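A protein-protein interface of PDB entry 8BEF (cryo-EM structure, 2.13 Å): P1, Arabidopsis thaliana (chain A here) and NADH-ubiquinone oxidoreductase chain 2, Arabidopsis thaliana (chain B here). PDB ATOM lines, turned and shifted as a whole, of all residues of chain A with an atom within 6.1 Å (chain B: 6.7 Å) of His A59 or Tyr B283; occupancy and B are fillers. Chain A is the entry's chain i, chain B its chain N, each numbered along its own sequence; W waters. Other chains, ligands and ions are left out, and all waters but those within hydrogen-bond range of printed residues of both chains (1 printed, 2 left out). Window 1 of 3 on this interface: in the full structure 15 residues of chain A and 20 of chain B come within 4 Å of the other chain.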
ATOM      1  N   PHE A  53      34.704  23.917 -20.725  1.00  0.00           N
ATOM      2  CA  PHE A  53      34.206  22.650 -21.250  1.00  0.00           C
ATOM      3  C   PHE A  53      33.598  22.830 -22.637  1.00  0.00           C
ATOM      4  O   PHE A  53      33.750  21.965 -23.505  1.00  0.00           O
ATOM      5  CB  PHE A  53      33.187  22.037 -20.291  1.00  0.00           C
ATOM      6  CG  PHE A  53      31.969  22.885 -20.067  1.00  0.00           C
ATOM      7  CD1 PHE A  53      31.968  23.885 -19.111  1.00  0.00           C
ATOM      8  CD2 PHE A  53      30.819  22.678 -20.809  1.00  0.00           C
ATOM      9  CE1 PHE A  53      30.844  24.662 -18.906  1.00  0.00           C
ATOM     10  CE2 PHE A  53      29.697  23.454 -20.607  1.00  0.00           C
ATOM     11  CZ  PHE A  53      29.708  24.444 -19.656  1.00  0.00           C
ATOM     12  N   TRP A  54      32.931  23.963 -22.873  1.00  0.00           N
ATOM     13  CA  TRP A  54      32.326  24.238 -24.171  1.00  0.00           C
ATOM     14  C   TRP A  54      33.357  24.357 -25.287  1.00  0.00           C
ATOM     15  O   TRP A  54      32.975  24.342 -26.462  1.00  0.00           O
ATOM     16  CB  TRP A  54      31.484  25.513 -24.089  1.00  0.00           C
ATOM     17  CG  TRP A  54      32.296  26.705 -23.722  1.00  0.00           C
ATOM     18  CD1 TRP A  54      32.957  27.530 -24.569  1.00  0.00           C
ATOM     19  CD2 TRP A  54      32.562  27.189 -22.400  1.00  0.00           C
ATOM     20  NE1 TRP A  54      33.615  28.510 -23.864  1.00  0.00           N
ATOM     21  CE2 TRP A  54      33.387  28.321 -22.528  1.00  0.00           C
ATOM     22  CE3 TRP A  54      32.178  26.776 -21.122  1.00  0.00           C
ATOM     23  CZ2 TRP A  54      33.830  29.048 -21.427  1.00  0.00           C
ATOM     24  CZ3 TRP A  54      32.621  27.497 -20.030  1.00  0.00           C
ATOM     25  CH2 TRP A  54      33.439  28.621 -20.190  1.00  0.00           C
ATOM     26  N   THR A  55      34.642  24.488 -24.951  1.00  0.00           N
ATOM     27  CA  THR A  55      35.713  24.418 -25.938  1.00  0.00           C
ATOM     28  C   THR A  55      35.937  23.003 -26.462  1.00  0.00           C
ATOM     29  O   THR A  55      36.412  22.844 -27.593  1.00  0.00           O
ATOM     30  CB  THR A  55      37.009  24.963 -25.323  1.00  0.00           C
ATOM     31  OG1 THR A  55      36.782  26.290 -24.835  1.00  0.00           O
ATOM     32  CG2 THR A  55      38.148  24.986 -26.332  1.00  0.00           C
ATOM     33  N   PHE A  56      35.606  21.967 -25.669  1.00  0.00           N
ATOM     34  CA  PHE A  56      35.854  20.554 -26.013  1.00  0.00           C
ATOM     35  C   PHE A  56      35.102  20.185 -27.314  1.00  0.00           C
ATOM     36  O   PHE A  56      33.922  20.558 -27.442  1.00  0.00           O
ATOM     37  CB  PHE A  56      35.546  19.673 -24.812  1.00  0.00           C
ATOM     38  CG  PHE A  56      36.198  19.990 -23.492  1.00  0.00           C
ATOM     39  CD1 PHE A  56      37.361  20.734 -23.412  1.00  0.00           C
ATOM     40  CD2 PHE A  56      35.630  19.535 -22.314  1.00  0.00           C
ATOM     41  CE1 PHE A  56      37.933  21.025 -22.185  1.00  0.00           C
ATOM     42  CE2 PHE A  56      36.195  19.838 -21.084  1.00  0.00           C
ATOM     43  CZ  PHE A  56      37.349  20.577 -21.027  1.00  0.00           C
ATOM     44  N   GLU A  57      35.756  19.487 -28.234  1.00  0.00           N
ATOM     45  CA  GLU A  57      35.266  19.265 -29.591  1.00  0.00           C
ATOM     46  C   GLU A  57      33.859  18.684 -29.611  1.00  0.00           C
ATOM     47  O   GLU A  57      33.076  18.997 -30.514  1.00  0.00           O
ATOM     48  CB  GLU A  57      36.225  18.346 -30.348  1.00  0.00           C
ATOM     49  CG  GLU A  57      37.464  19.048 -30.879  1.00  0.00           C
ATOM     50  CD  GLU A  57      38.467  19.371 -29.786  1.00  0.00           C
ATOM     51  OE1 GLU A  57      38.374  18.772 -28.694  1.00  0.00           O
ATOM     52  OE2 GLU A  57      39.350  20.224 -30.020  1.00  0.00           O
ATOM     53  N   ARG A  58      33.519  17.839 -28.632  1.00  0.00           N
ATOM     54  CA  ARG A  58      32.173  17.281 -28.571  1.00  0.00           C
ATOM     55  C   ARG A  58      31.112  18.376 -28.513  1.00  0.00           C
ATOM     56  O   ARG A  58      29.991  18.183 -28.995  1.00  0.00           O
ATOM     57  CB  ARG A  58      32.047  16.349 -27.364  1.00  0.00           C
ATOM     58  CG  ARG A  58      30.624  15.921 -27.030  1.00  0.00           C
ATOM     59  CD  ARG A  58      30.064  14.979 -28.086  1.00  0.00           C
ATOM     60  NE  ARG A  58      29.382  15.683 -29.165  1.00  0.00           N
ATOM     61  CZ  ARG A  58      28.955  15.107 -30.281  1.00  0.00           C
ATOM     62  NH1 ARG A  58      29.115  13.813 -30.496  1.00  0.00           N
ATOM     63  NH2 ARG A  58      28.351  15.849 -31.205  1.00  0.00           N
ATOM     64  N   HIS A  59      31.484  19.534 -27.988  1.00  0.00           N
ATOM     65  CA  HIS A  59      30.493  20.604 -27.794  1.00  0.00           C
ATOM     66  C   HIS A  59      30.447  21.598 -28.975  1.00  0.00           C
ATOM     67  O   HIS A  59      29.642  22.498 -28.958  1.00  0.00           O
ATOM     68  CB  HIS A  59      30.818  21.232 -26.474  1.00  0.00           C
ATOM     69  CG  HIS A  59      30.969  20.308 -25.306  1.00  0.00           C
ATOM     70  ND1 HIS A  59      31.233  20.778 -24.045  1.00  0.00           N
ATOM     71  CD2 HIS A  59      30.920  18.963 -25.193  1.00  0.00           C
ATOM     72  CE1 HIS A  59      31.340  19.772 -23.207  1.00  0.00           C
ATOM     73  NE2 HIS A  59      31.158  18.646 -23.887  1.00  0.00           N
ATOM     74  N   ASN A  60      31.338  21.450 -29.926  1.00  0.00           N
ATOM     75  CA  ASN A  60      31.396  22.344 -31.076  1.00  0.00           C
ATOM     76  C   ASN A  60      30.812  21.681 -32.320  1.00  0.00           C
ATOM     77  O   ASN A  60      31.291  21.886 -33.436  1.00  0.00           O
ATOM     78  CB  ASN A  60      32.829  22.802 -31.336  1.00  0.00           C
ATOM     79  CG  ASN A  60      33.343  23.747 -30.266  1.00  0.00           C
ATOM     80  OD1 ASN A  60      32.567  24.412 -29.579  1.00  0.00           O
ATOM     81  ND2 ASN A  60      34.664  23.811 -30.121  1.00  0.00           N
ATOM     82  N   ALA A  61      29.769  20.872 -32.132  1.00  0.00           N
ATOM     83  CA  ALA A  61      29.197  20.130 -33.251  1.00  0.00           C
ATOM     84  C   ALA A  61      28.645  21.064 -34.323  1.00  0.00           C
ATOM     85  O   ALA A  61      28.851  20.831 -35.518  1.00  0.00           O
ATOM     86  CB  ALA A  61      28.107  19.182 -32.749  1.00  0.00           C
ATOM     87  N   GLN A  62      27.949  22.131 -33.919  1.00  0.00           N
ATOM     88  CA  GLN A  62      27.326  23.011 -34.904  1.00  0.00           C
ATOM     89  C   GLN A  62      28.374  23.757 -35.727  1.00  0.00           C
ATOM     90  O   GLN A  62      28.181  23.984 -36.925  1.00  0.00           O
ATOM     91  CB  GLN A  62      26.366  23.987 -34.216  1.00  0.00           C
ATOM     92  CG  GLN A  62      25.898  25.140 -35.102  1.00  0.00           C
ATOM     93  CD  GLN A  62      24.823  26.006 -34.456  1.00  0.00           C
ATOM     94  OE1 GLN A  62      24.841  26.249 -33.252  1.00  0.00           O
ATOM     95  NE2 GLN A  62      23.886  26.481 -35.266  1.00  0.00           N
ATOM     96  N   ARG A  64      30.998  22.653 -36.910  1.00  0.00           N
ATOM     97  CA  ARG A  64      31.503  21.789 -37.968  1.00  0.00           C
ATOM     98  C   ARG A  64      30.416  21.264 -38.892  1.00  0.00           C
ATOM     99  O   ARG A  64      30.716  20.926 -40.041  1.00  0.00           O
ATOM    100  CB  ARG A  64      32.262  20.603 -37.367  1.00  0.00           C
ATOM    101  CG  ARG A  64      33.129  20.972 -36.183  1.00  0.00           C
ATOM    102  CD  ARG A  64      34.358  20.086 -36.109  1.00  0.00           C
ATOM    103  NE  ARG A  64      34.023  18.697 -35.814  1.00  0.00           N
ATOM    104  CZ  ARG A  64      33.565  18.264 -34.648  1.00  0.00           C
ATOM    105  NH1 ARG A  64      33.364  19.088 -33.632  1.00  0.00           N
ATOM    106  NH2 ARG A  64      33.304  16.970 -34.494  1.00  0.00           N
ATOM    107  N   ARG B  88      21.998  12.982 -29.072  1.00  0.00           N
ATOM    108  CA  ARG B  88      23.422  12.891 -28.758  1.00  0.00           C
ATOM    109  C   ARG B  88      23.673  11.632 -27.944  1.00  0.00           C
ATOM    110  O   ARG B  88      23.175  11.512 -26.821  1.00  0.00           O
ATOM    111  CB  ARG B  88      23.905  14.120 -27.983  1.00  0.00           C
ATOM    112  CG  ARG B  88      25.413  14.160 -27.788  1.00  0.00           C
ATOM    113  CD  ARG B  88      25.890  15.543 -27.401  1.00  0.00           C
ATOM    114  NE  ARG B  88      26.033  16.416 -28.560  1.00  0.00           N
ATOM    115  CZ  ARG B  88      26.667  17.578 -28.545  1.00  0.00           C
ATOM    116  NH1 ARG B  88      27.254  18.030 -27.448  1.00  0.00           N
ATOM    117  NH2 ARG B  88      26.704  18.311 -29.653  1.00  0.00           N
ATOM    118  N   ASP B  90      26.435   9.143 -26.084  1.00  0.00           N
ATOM    119  CA  ASP B  90      27.782   9.073 -25.521  1.00  0.00           C
ATOM    120  C   ASP B  90      27.813   7.968 -24.466  1.00  0.00           C
ATOM    121  O   ASP B  90      26.892   7.151 -24.373  1.00  0.00           O
ATOM    122  CB  ASP B  90      28.216  10.435 -24.962  1.00  0.00           C
ATOM    123  CG  ASP B  90      27.122  11.131 -24.178  1.00  0.00           C
ATOM    124  OD1 ASP B  90      26.390  10.456 -23.424  1.00  0.00           O
ATOM    125  OD2 ASP B  90      26.998  12.365 -24.315  1.00  0.00           O
ATOM    126  N   TYR B 143      18.849  15.767 -26.768  1.00  0.00           N
ATOM    127  CA  TYR B 143      19.810  16.848 -26.591  1.00  0.00           C
ATOM    128  C   TYR B 143      19.227  18.181 -27.055  1.00  0.00           C
ATOM    129  O   TYR B 143      19.966  19.090 -27.444  1.00  0.00           O
ATOM    130  CB  TYR B 143      21.115  16.535 -27.321  1.00  0.00           C
ATOM    131  CG  TYR B 143      22.329  17.136 -26.660  1.00  0.00           C
ATOM    132  CD1 TYR B 143      22.697  16.779 -25.367  1.00  0.00           C
ATOM    133  CD2 TYR B 143      23.103  18.069 -27.326  1.00  0.00           C
ATOM    134  CE1 TYR B 143      23.806  17.343 -24.761  1.00  0.00           C
ATOM    135  CE2 TYR B 143      24.201  18.636 -26.735  1.00  0.00           C
ATOM    136  CZ  TYR B 143      24.555  18.271 -25.458  1.00  0.00           C
ATOM    137  OH  TYR B 143      25.660  18.851 -24.894  1.00  0.00           O
ATOM    138  N   PHE B 206      20.841  21.840 -26.723  1.00  0.00           N
ATOM    139  CA  PHE B 206      21.481  21.932 -25.411  1.00  0.00           C
ATOM    140  C   PHE B 206      22.854  22.597 -25.497  1.00  0.00           C
ATOM    141  O   PHE B 206      23.249  23.327 -24.584  1.00  0.00           O
ATOM    142  CB  PHE B 206      21.595  20.547 -24.767  1.00  0.00           C
ATOM    143  CG  PHE B 206      20.283  19.983 -24.277  1.00  0.00           C
ATOM    144  CD1 PHE B 206      19.094  20.679 -24.450  1.00  0.00           C
ATOM    145  CD2 PHE B 206      20.242  18.754 -23.637  1.00  0.00           C
ATOM    146  CE1 PHE B 206      17.894  20.161 -24.006  1.00  0.00           C
ATOM    147  CE2 PHE B 206      19.041  18.229 -23.190  1.00  0.00           C
ATOM    148  CZ  PHE B 206      17.865  18.934 -23.380  1.00  0.00           C
ATOM    149  N   ASP B 207      23.596  22.352 -26.579  1.00  0.00           N
ATOM    150  CA  ASP B 207      24.902  22.990 -26.747  1.00  0.00           C
ATOM    151  C   ASP B 207      24.767  24.505 -26.830  1.00  0.00           C
ATOM    152  O   ASP B 207      25.507  25.250 -26.171  1.00  0.00           O
ATOM    153  CB  ASP B 207      25.588  22.459 -28.004  1.00  0.00           C
ATOM    154  CG  ASP B 207      26.443  21.250 -27.735  1.00  0.00           C
ATOM    155  OD1 ASP B 207      26.789  20.549 -28.707  1.00  0.00           O
ATOM    156  OD2 ASP B 207      26.763  20.992 -26.558  1.00  0.00           O
ATOM    157  N   GLN B 208      23.823  24.977 -27.648  1.00  0.00           N
ATOM    158  CA  GLN B 208      23.599  26.411 -27.785  1.00  0.00           C
ATOM    159  C   GLN B 208      23.185  27.026 -26.456  1.00  0.00           C
ATOM    160  O   GLN B 208      23.669  28.098 -26.081  1.00  0.00           O
ATOM    161  CB  GLN B 208      22.535  26.672 -28.851  1.00  0.00           C
ATOM    162  CG  GLN B 208      22.826  26.046 -30.207  1.00  0.00           C
ATOM    163  CD  GLN B 208      21.613  26.034 -31.124  1.00  0.00           C
ATOM    164  OE1 GLN B 208      20.472  26.064 -30.665  1.00  0.00           O
ATOM    165  NE2 GLN B 208      21.857  25.993 -32.428  1.00  0.00           N
ATOM    166  N   LEU B 209      22.291  26.353 -25.729  1.00  0.00           N
ATOM    167  CA  LEU B 209      21.872  26.842 -24.422  1.00  0.00           C
ATOM    168  C   LEU B 209      23.048  26.912 -23.460  1.00  0.00           C
ATOM    169  O   LEU B 209      23.176  27.873 -22.693  1.00  0.00           O
ATOM    170  CB  LEU B 209      20.770  25.947 -23.859  1.00  0.00           C
ATOM    171  CG  LEU B 209      19.447  25.993 -24.630  1.00  0.00           C
ATOM    172  CD1 LEU B 209      18.420  25.040 -24.022  1.00  0.00           C
ATOM    173  CD2 LEU B 209      18.918  27.415 -24.677  1.00  0.00           C
ATOM    174  N   ALA B 210      23.924  25.906 -23.491  1.00  0.00           N
ATOM    175  CA  ALA B 210      25.108  25.935 -22.643  1.00  0.00           C
ATOM    176  C   ALA B 210      25.980  27.142 -22.970  1.00  0.00           C
ATOM    177  O   ALA B 210      26.410  27.868 -22.071  1.00  0.00           O
ATOM    178  CB  ALA B 210      25.898  24.632 -22.796  1.00  0.00           C
ATOM    179  N   LYS B 211      26.224  27.391 -24.259  1.00  0.00           N
ATOM    180  CA  LYS B 211      27.076  28.520 -24.630  1.00  0.00           C
ATOM    181  C   LYS B 211      26.466  29.853 -24.205  1.00  0.00           C
ATOM    182  O   LYS B 211      27.165  30.714 -23.659  1.00  0.00           O
ATOM    183  CB  LYS B 211      27.348  28.512 -26.132  1.00  0.00           C
ATOM    184  CG  LYS B 211      28.473  27.585 -26.547  1.00  0.00           C
ATOM    185  CD  LYS B 211      28.477  27.361 -28.047  1.00  0.00           C
ATOM    186  CE  LYS B 211      29.774  26.724 -28.509  1.00  0.00           C
ATOM    187  NZ  LYS B 211      29.944  25.360 -27.947  1.00  0.00           N
ATOM    188  N   THR B 214      26.318  30.195 -20.077  1.00  0.00           N
ATOM    189  CA  THR B 214      27.512  30.043 -19.255  1.00  0.00           C
ATOM    190  C   THR B 214      28.226  31.374 -19.075  1.00  0.00           C
ATOM    191  O   THR B 214      28.311  32.183 -20.002  1.00  0.00           O
ATOM    192  CB  THR B 214      28.480  29.026 -19.862  1.00  0.00           C
ATOM    193  OG1 THR B 214      28.504  29.165 -21.286  1.00  0.00           O
ATOM    194  CG2 THR B 214      28.068  27.610 -19.486  1.00  0.00           C
ATOM    195  N   ILE B 277      17.440  15.242 -16.550  1.00  0.00           N
ATOM    196  CA  ILE B 277      17.729  16.322 -15.610  1.00  0.00           C
ATOM    197  C   ILE B 277      19.223  16.609 -15.583  1.00  0.00           C
ATOM    198  O   ILE B 277      19.653  17.770 -15.625  1.00  0.00           O
ATOM    199  CB  ILE B 277      17.197  15.974 -14.207  1.00  0.00           C
ATOM    200  CG1 ILE B 277      15.668  16.004 -14.178  1.00  0.00           C
ATOM    201  CG2 ILE B 277      17.764  16.919 -13.160  1.00  0.00           C
ATOM    202  CD1 ILE B 277      15.069  15.203 -13.053  1.00  0.00           C
ATOM    203  N   LEU B 278      20.036  15.552 -15.517  1.00  0.00           N
ATOM    204  CA  LEU B 278      21.482  15.723 -15.568  1.00  0.00           C
ATOM    205  C   LEU B 278      21.884  16.503 -16.812  1.00  0.00           C
ATOM    206  O   LEU B 278      22.482  17.581 -16.712  1.00  0.00           O
ATOM    207  CB  LEU B 278      22.173  14.356 -15.528  1.00  0.00           C
ATOM    208  CG  LEU B 278      22.059  13.537 -14.233  1.00  0.00           C
ATOM    209  CD1 LEU B 278      23.176  12.516 -14.109  1.00  0.00           C
ATOM    210  CD2 LEU B 278      22.040  14.437 -13.016  1.00  0.00           C
ATOM    211  N   ARG B 279      21.444  16.034 -17.987  1.00  0.00           N
ATOM    212  CA  ARG B 279      21.893  16.636 -19.239  1.00  0.00           C
ATOM    213  C   ARG B 279      21.317  18.024 -19.485  1.00  0.00           C
ATOM    214  O   ARG B 279      21.893  18.786 -20.266  1.00  0.00           O
ATOM    215  CB  ARG B 279      21.550  15.734 -20.419  1.00  0.00           C
ATOM    216  CG  ARG B 279      22.293  14.422 -20.428  1.00  0.00           C
ATOM    217  CD  ARG B 279      22.005  13.658 -21.700  1.00  0.00           C
ATOM    218  NE  ARG B 279      23.191  13.544 -22.538  1.00  0.00           N
ATOM    219  CZ  ARG B 279      23.162  13.280 -23.836  1.00  0.00           C
ATOM    220  NH1 ARG B 279      22.018  13.121 -24.480  1.00  0.00           N
ATOM    221  NH2 ARG B 279      24.307  13.176 -24.503  1.00  0.00           N
ATOM    222  N   VAL B 280      20.190  18.368 -18.876  1.00  0.00           N
ATOM    223  CA  VAL B 280      19.651  19.713 -19.030  1.00  0.00           C
ATOM    224  C   VAL B 280      20.322  20.677 -18.067  1.00  0.00           C
ATOM    225  O   VAL B 280      20.994  21.627 -18.480  1.00  0.00           O
ATOM    226  CB  VAL B 280      18.119  19.706 -18.830  1.00  0.00           C
ATOM    227  CG1 VAL B 280      17.605  21.118 -18.659  1.00  0.00           C
ATOM    228  CG2 VAL B 280      17.424  19.031 -19.988  1.00  0.00           C
ATOM    229  N   PHE B 281      20.199  20.412 -16.769  1.00  0.00           N
ATOM    230  CA  PHE B 281      20.634  21.362 -15.760  1.00  0.00           C
ATOM    231  C   PHE B 281      22.141  21.346 -15.541  1.00  0.00           C
ATOM    232  O   PHE B 281      22.784  22.398 -15.606  1.00  0.00           O
ATOM    233  CB  PHE B 281      19.901  21.090 -14.447  1.00  0.00           C
ATOM    234  CG  PHE B 281      18.405  21.180 -14.561  1.00  0.00           C
ATOM    235  CD1 PHE B 281      17.820  22.070 -15.446  1.00  0.00           C
ATOM    236  CD2 PHE B 281      17.585  20.426 -13.743  1.00  0.00           C
ATOM    237  CE1 PHE B 281      16.450  22.182 -15.543  1.00  0.00           C
ATOM    238  CE2 PHE B 281      16.213  20.534 -13.831  1.00  0.00           C
ATOM    239  CZ  PHE B 281      15.645  21.418 -14.735  1.00  0.00           C
ATOM    240  N   ILE B 282      22.640  20.239 -15.009  1.00  0.00           N
ATOM    241  CA  ILE B 282      24.103  19.988 -14.866  1.00  0.00           C
ATOM    242  C   ILE B 282      24.926  20.444 -16.090  1.00  0.00           C
ATOM    243  O   ILE B 282      25.941  21.131 -15.833  1.00  0.00           O
ATOM    244  CB  ILE B 282      24.255  18.467 -14.545  1.00  0.00           C
ATOM    245  CG1 ILE B 282      24.060  18.130 -13.066  1.00  0.00           C
ATOM    246  CG2 ILE B 282      25.544  17.900 -15.116  1.00  0.00           C
ATOM    247  CD1 ILE B 282      25.277  18.385 -12.221  1.00  0.00           C
ATOM    248  N   TYR B 283      24.490  20.233 -17.344  1.00  0.00           N
ATOM    249  CA  TYR B 283      25.176  20.536 -18.585  1.00  0.00           C
ATOM    250  C   TYR B 283      24.883  21.959 -19.056  1.00  0.00           C
ATOM    251  O   TYR B 283      25.661  22.512 -19.842  1.00  0.00           O
ATOM    252  CB  TYR B 283      24.743  19.499 -19.619  1.00  0.00           C
ATOM    253  CG  TYR B 283      25.745  19.114 -20.674  1.00  0.00           C
ATOM    254  CD1 TYR B 283      26.897  19.852 -20.898  1.00  0.00           C
ATOM    255  CD2 TYR B 283      25.558  17.947 -21.402  1.00  0.00           C
ATOM    256  CE1 TYR B 283      27.815  19.453 -21.858  1.00  0.00           C
ATOM    257  CE2 TYR B 283      26.460  17.539 -22.344  1.00  0.00           C
ATOM    258  CZ  TYR B 283      27.583  18.290 -22.577  1.00  0.00           C
ATOM    259  OH  TYR B 283      28.467  17.857 -23.534  1.00  0.00           O
ATOM    260  N   GLY B 284      23.870  22.563 -18.433  1.00  0.00           N
ATOM    261  CA  GLY B 284      23.406  23.924 -18.783  1.00  0.00           C
ATOM    262  C   GLY B 284      23.843  24.941 -17.756  1.00  0.00           C
ATOM    263  O   GLY B 284      24.810  24.638 -17.052  1.00  0.00           O
ATOM    264  N   SER B 285      23.133  26.070 -17.642  1.00  0.00           N
ATOM    265  CA  SER B 285      23.640  27.075 -16.676  1.00  0.00           C
ATOM    266  C   SER B 285      22.715  28.166 -16.203  1.00  0.00           C
ATOM    267  O   SER B 285      22.706  29.190 -16.860  1.00  0.00           O
ATOM    268  CB  SER B 285      24.863  27.725 -17.194  1.00  0.00           C
ATOM    269  OG  SER B 285      26.017  26.954 -16.878  1.00  0.00           O
ATOM    270  N   SER B 496      31.663  11.682 -17.961  1.00  0.00           N
ATOM    271  CA  SER B 496      31.263  11.766 -19.386  1.00  0.00           C
ATOM    272  C   SER B 496      30.236  12.880 -19.660  1.00  0.00           C
ATOM    273  O   SER B 496      30.201  13.308 -20.788  1.00  0.00           O
ATOM    274  CB  SER B 496      30.785  10.393 -19.897  1.00  0.00           C
ATOM    275  OG  SER B 496      31.737   9.377 -19.657  1.00  0.00           O
ATOM    276  N   LEU B 497      29.487  13.345 -18.662  1.00  0.00           N
ATOM    277  CA  LEU B 497      28.541  14.487 -18.795  1.00  0.00           C
ATOM    278  C   LEU B 497      29.284  15.741 -19.293  1.00  0.00           C
ATOM    279  O   LEU B 497      28.757  16.400 -20.128  1.00  0.00           O
ATOM    280  CB  LEU B 497      27.924  14.727 -17.419  1.00  0.00           C
ATOM    281  CG  LEU B 497      26.764  13.815 -17.029  1.00  0.00           C
ATOM    282  CD1 LEU B 497      26.279  14.122 -15.622  1.00  0.00           C
ATOM    283  CD2 LEU B 497      25.620  13.905 -18.026  1.00  0.00           C
ATOM    284  N   TYR B 498      30.542  15.926 -18.929  1.00  0.00           N
ATOM    285  CA  TYR B 498      31.314  17.156 -19.308  1.00  0.00           C
ATOM    286  C   TYR B 498      32.569  16.836 -20.092  1.00  0.00           C
ATOM    287  O   TYR B 498      33.320  17.725 -20.301  1.00  0.00           O
ATOM    288  CB  TYR B 498      31.826  17.802 -18.037  1.00  0.00           C
ATOM    289  CG  TYR B 498      30.872  17.716 -16.884  1.00  0.00           C
ATOM    290  CD1 TYR B 498      30.910  16.643 -16.015  1.00  0.00           C
ATOM    291  CD2 TYR B 498      29.898  18.680 -16.701  1.00  0.00           C
ATOM    292  CE1 TYR B 498      30.006  16.537 -14.975  1.00  0.00           C
ATOM    293  CE2 TYR B 498      28.998  18.596 -15.658  1.00  0.00           C
ATOM    294  CZ  TYR B 498      29.049  17.515 -14.800  1.00  0.00           C
ATOM    295  OH  TYR B 498      28.167  17.405 -13.769  1.00  0.00           O
ATOM    296  N   LEU B 499      32.828  15.583 -20.409  1.00  0.00           N
ATOM    297  CA  LEU B 499      34.112  15.159 -21.010  1.00  0.00           C
ATOM    298  C   LEU B 499      34.107  13.675 -21.243  1.00  0.00           C
ATOM    299  O   LEU B 499      34.709  13.238 -22.257  1.00  0.00           O
ATOM    300  CB  LEU B 499      35.240  15.469 -19.982  1.00  0.00           C
ATOM    301  CG  LEU B 499      35.353  14.536 -18.781  1.00  0.00           C
ATOM    302  CD1 LEU B 499      36.470  13.521 -18.965  1.00  0.00           C
ATOM    303  CD2 LEU B 499      35.570  15.333 -17.506  1.00  0.00           C
HETATM  304  O   HOH W   1      27.143  22.296 -31.241  1.00  0.00           O
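The guanidinium group (NH1) of Arg B88 sits at hydrogen-bond distance from the backbone carbonyl oxygen (O) of Arg A58 (3.1 Å). The backbone carbonyl oxygen of His A59 lies within hydrogen-bond range of the side-chain amino group of Lys B211 (3.1 Å). OH of Tyr B283 is in hydrogen-bond range of NE2 of His A59, 2.8 Å away. The side-chain amino group of Lys B211 sits at hydrogen-bond distance from the side-chain amide oxygen of Asn A60, 3.2 Å away. NE2 of Gln B208 is in hydrogen-bond range of OE1 of Gln A62. The backbone carbonyl oxygen (O) of His A59 lies close to the side-chain carboxylate (OD1) of Asp B207, at 3.5 Å.
A ring nitrogen (ND1) of His A59 sits at hydrogen-bond distance from the backbone carbonyl oxygen (O) of Phe A53 (2.8 Å). OD1 of Asn A60 sits close to O of Trp A54. ND2 of Asn A60 sits at hydrogen-bond distance from O of Thr A55 (3.2 Å). NH1 of Arg B88 sits at hydrogen-bond distance from OH of Tyr B143 (3.1 Å). The backbone carbonyl oxygen of Ala B210 is in hydrogen-bond range of the side-chain hydroxyl of Thr B214 (2.6 Å). The backbone carbonyl oxygen of Lys B211 is in hydrogen-bond range of the side-chain hydroxyl of Thr B214 (3.1 Å).
Among the printed residues, merely in contact across the chains: Ala A61 with Arg B88 (3.5 Å), Trp A54 with Lys B211 (3.5 Å), Phe A56 with Tyr B498 (3.6 Å), Phe A53 with Thr B214 (3.6 Å) and Arg A58 with Asp B207 (3.99 Å).
Of the printed residues of chain B, His A59 touches Asp B207 (3.5 Å), Lys B211 (3.1 Å) and Tyr B283 (2.8 Å). Tyr B283 touches one residue of chain A. Printed residues of chain A within 4 Å of Tyr B498: Phe A56 (3.6 Å). Printed residues of chain A within 4 Å of Gln B208: Gln A62 (3.1 Å). Of the printed residues of chain B, Asn A60 touches Lys B211. Tyr B143 touches none of the printed residues of chain A. The nearest residue of chain A that does not touch Tyr B283 is Phe A53 (4.2 Å).
Of the 11 printed residues of chain A, 8 touch a printed residue of chain B. Hydrophobic or aromatic side chains of chain A that line the printed part of chain B: Phe A53, Phe A56, His A59 and Ala A61. Of the 23 printed residues of chain B, 7 touch a printed residue of chain A. Hydrophobic or aromatic side chains of chain B that line the printed part of chain A: Tyr B283.
Water W1 lies within hydrogen-bond range of the backbone NH of Gln A62 (2.8 Å), the side-chain carboxylate of Asp B207 (3.1 Å), the backbone NH of Ala A61 (3.1 Å) and the backbone carbonyl oxygen of His A59 (3.4 Å).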
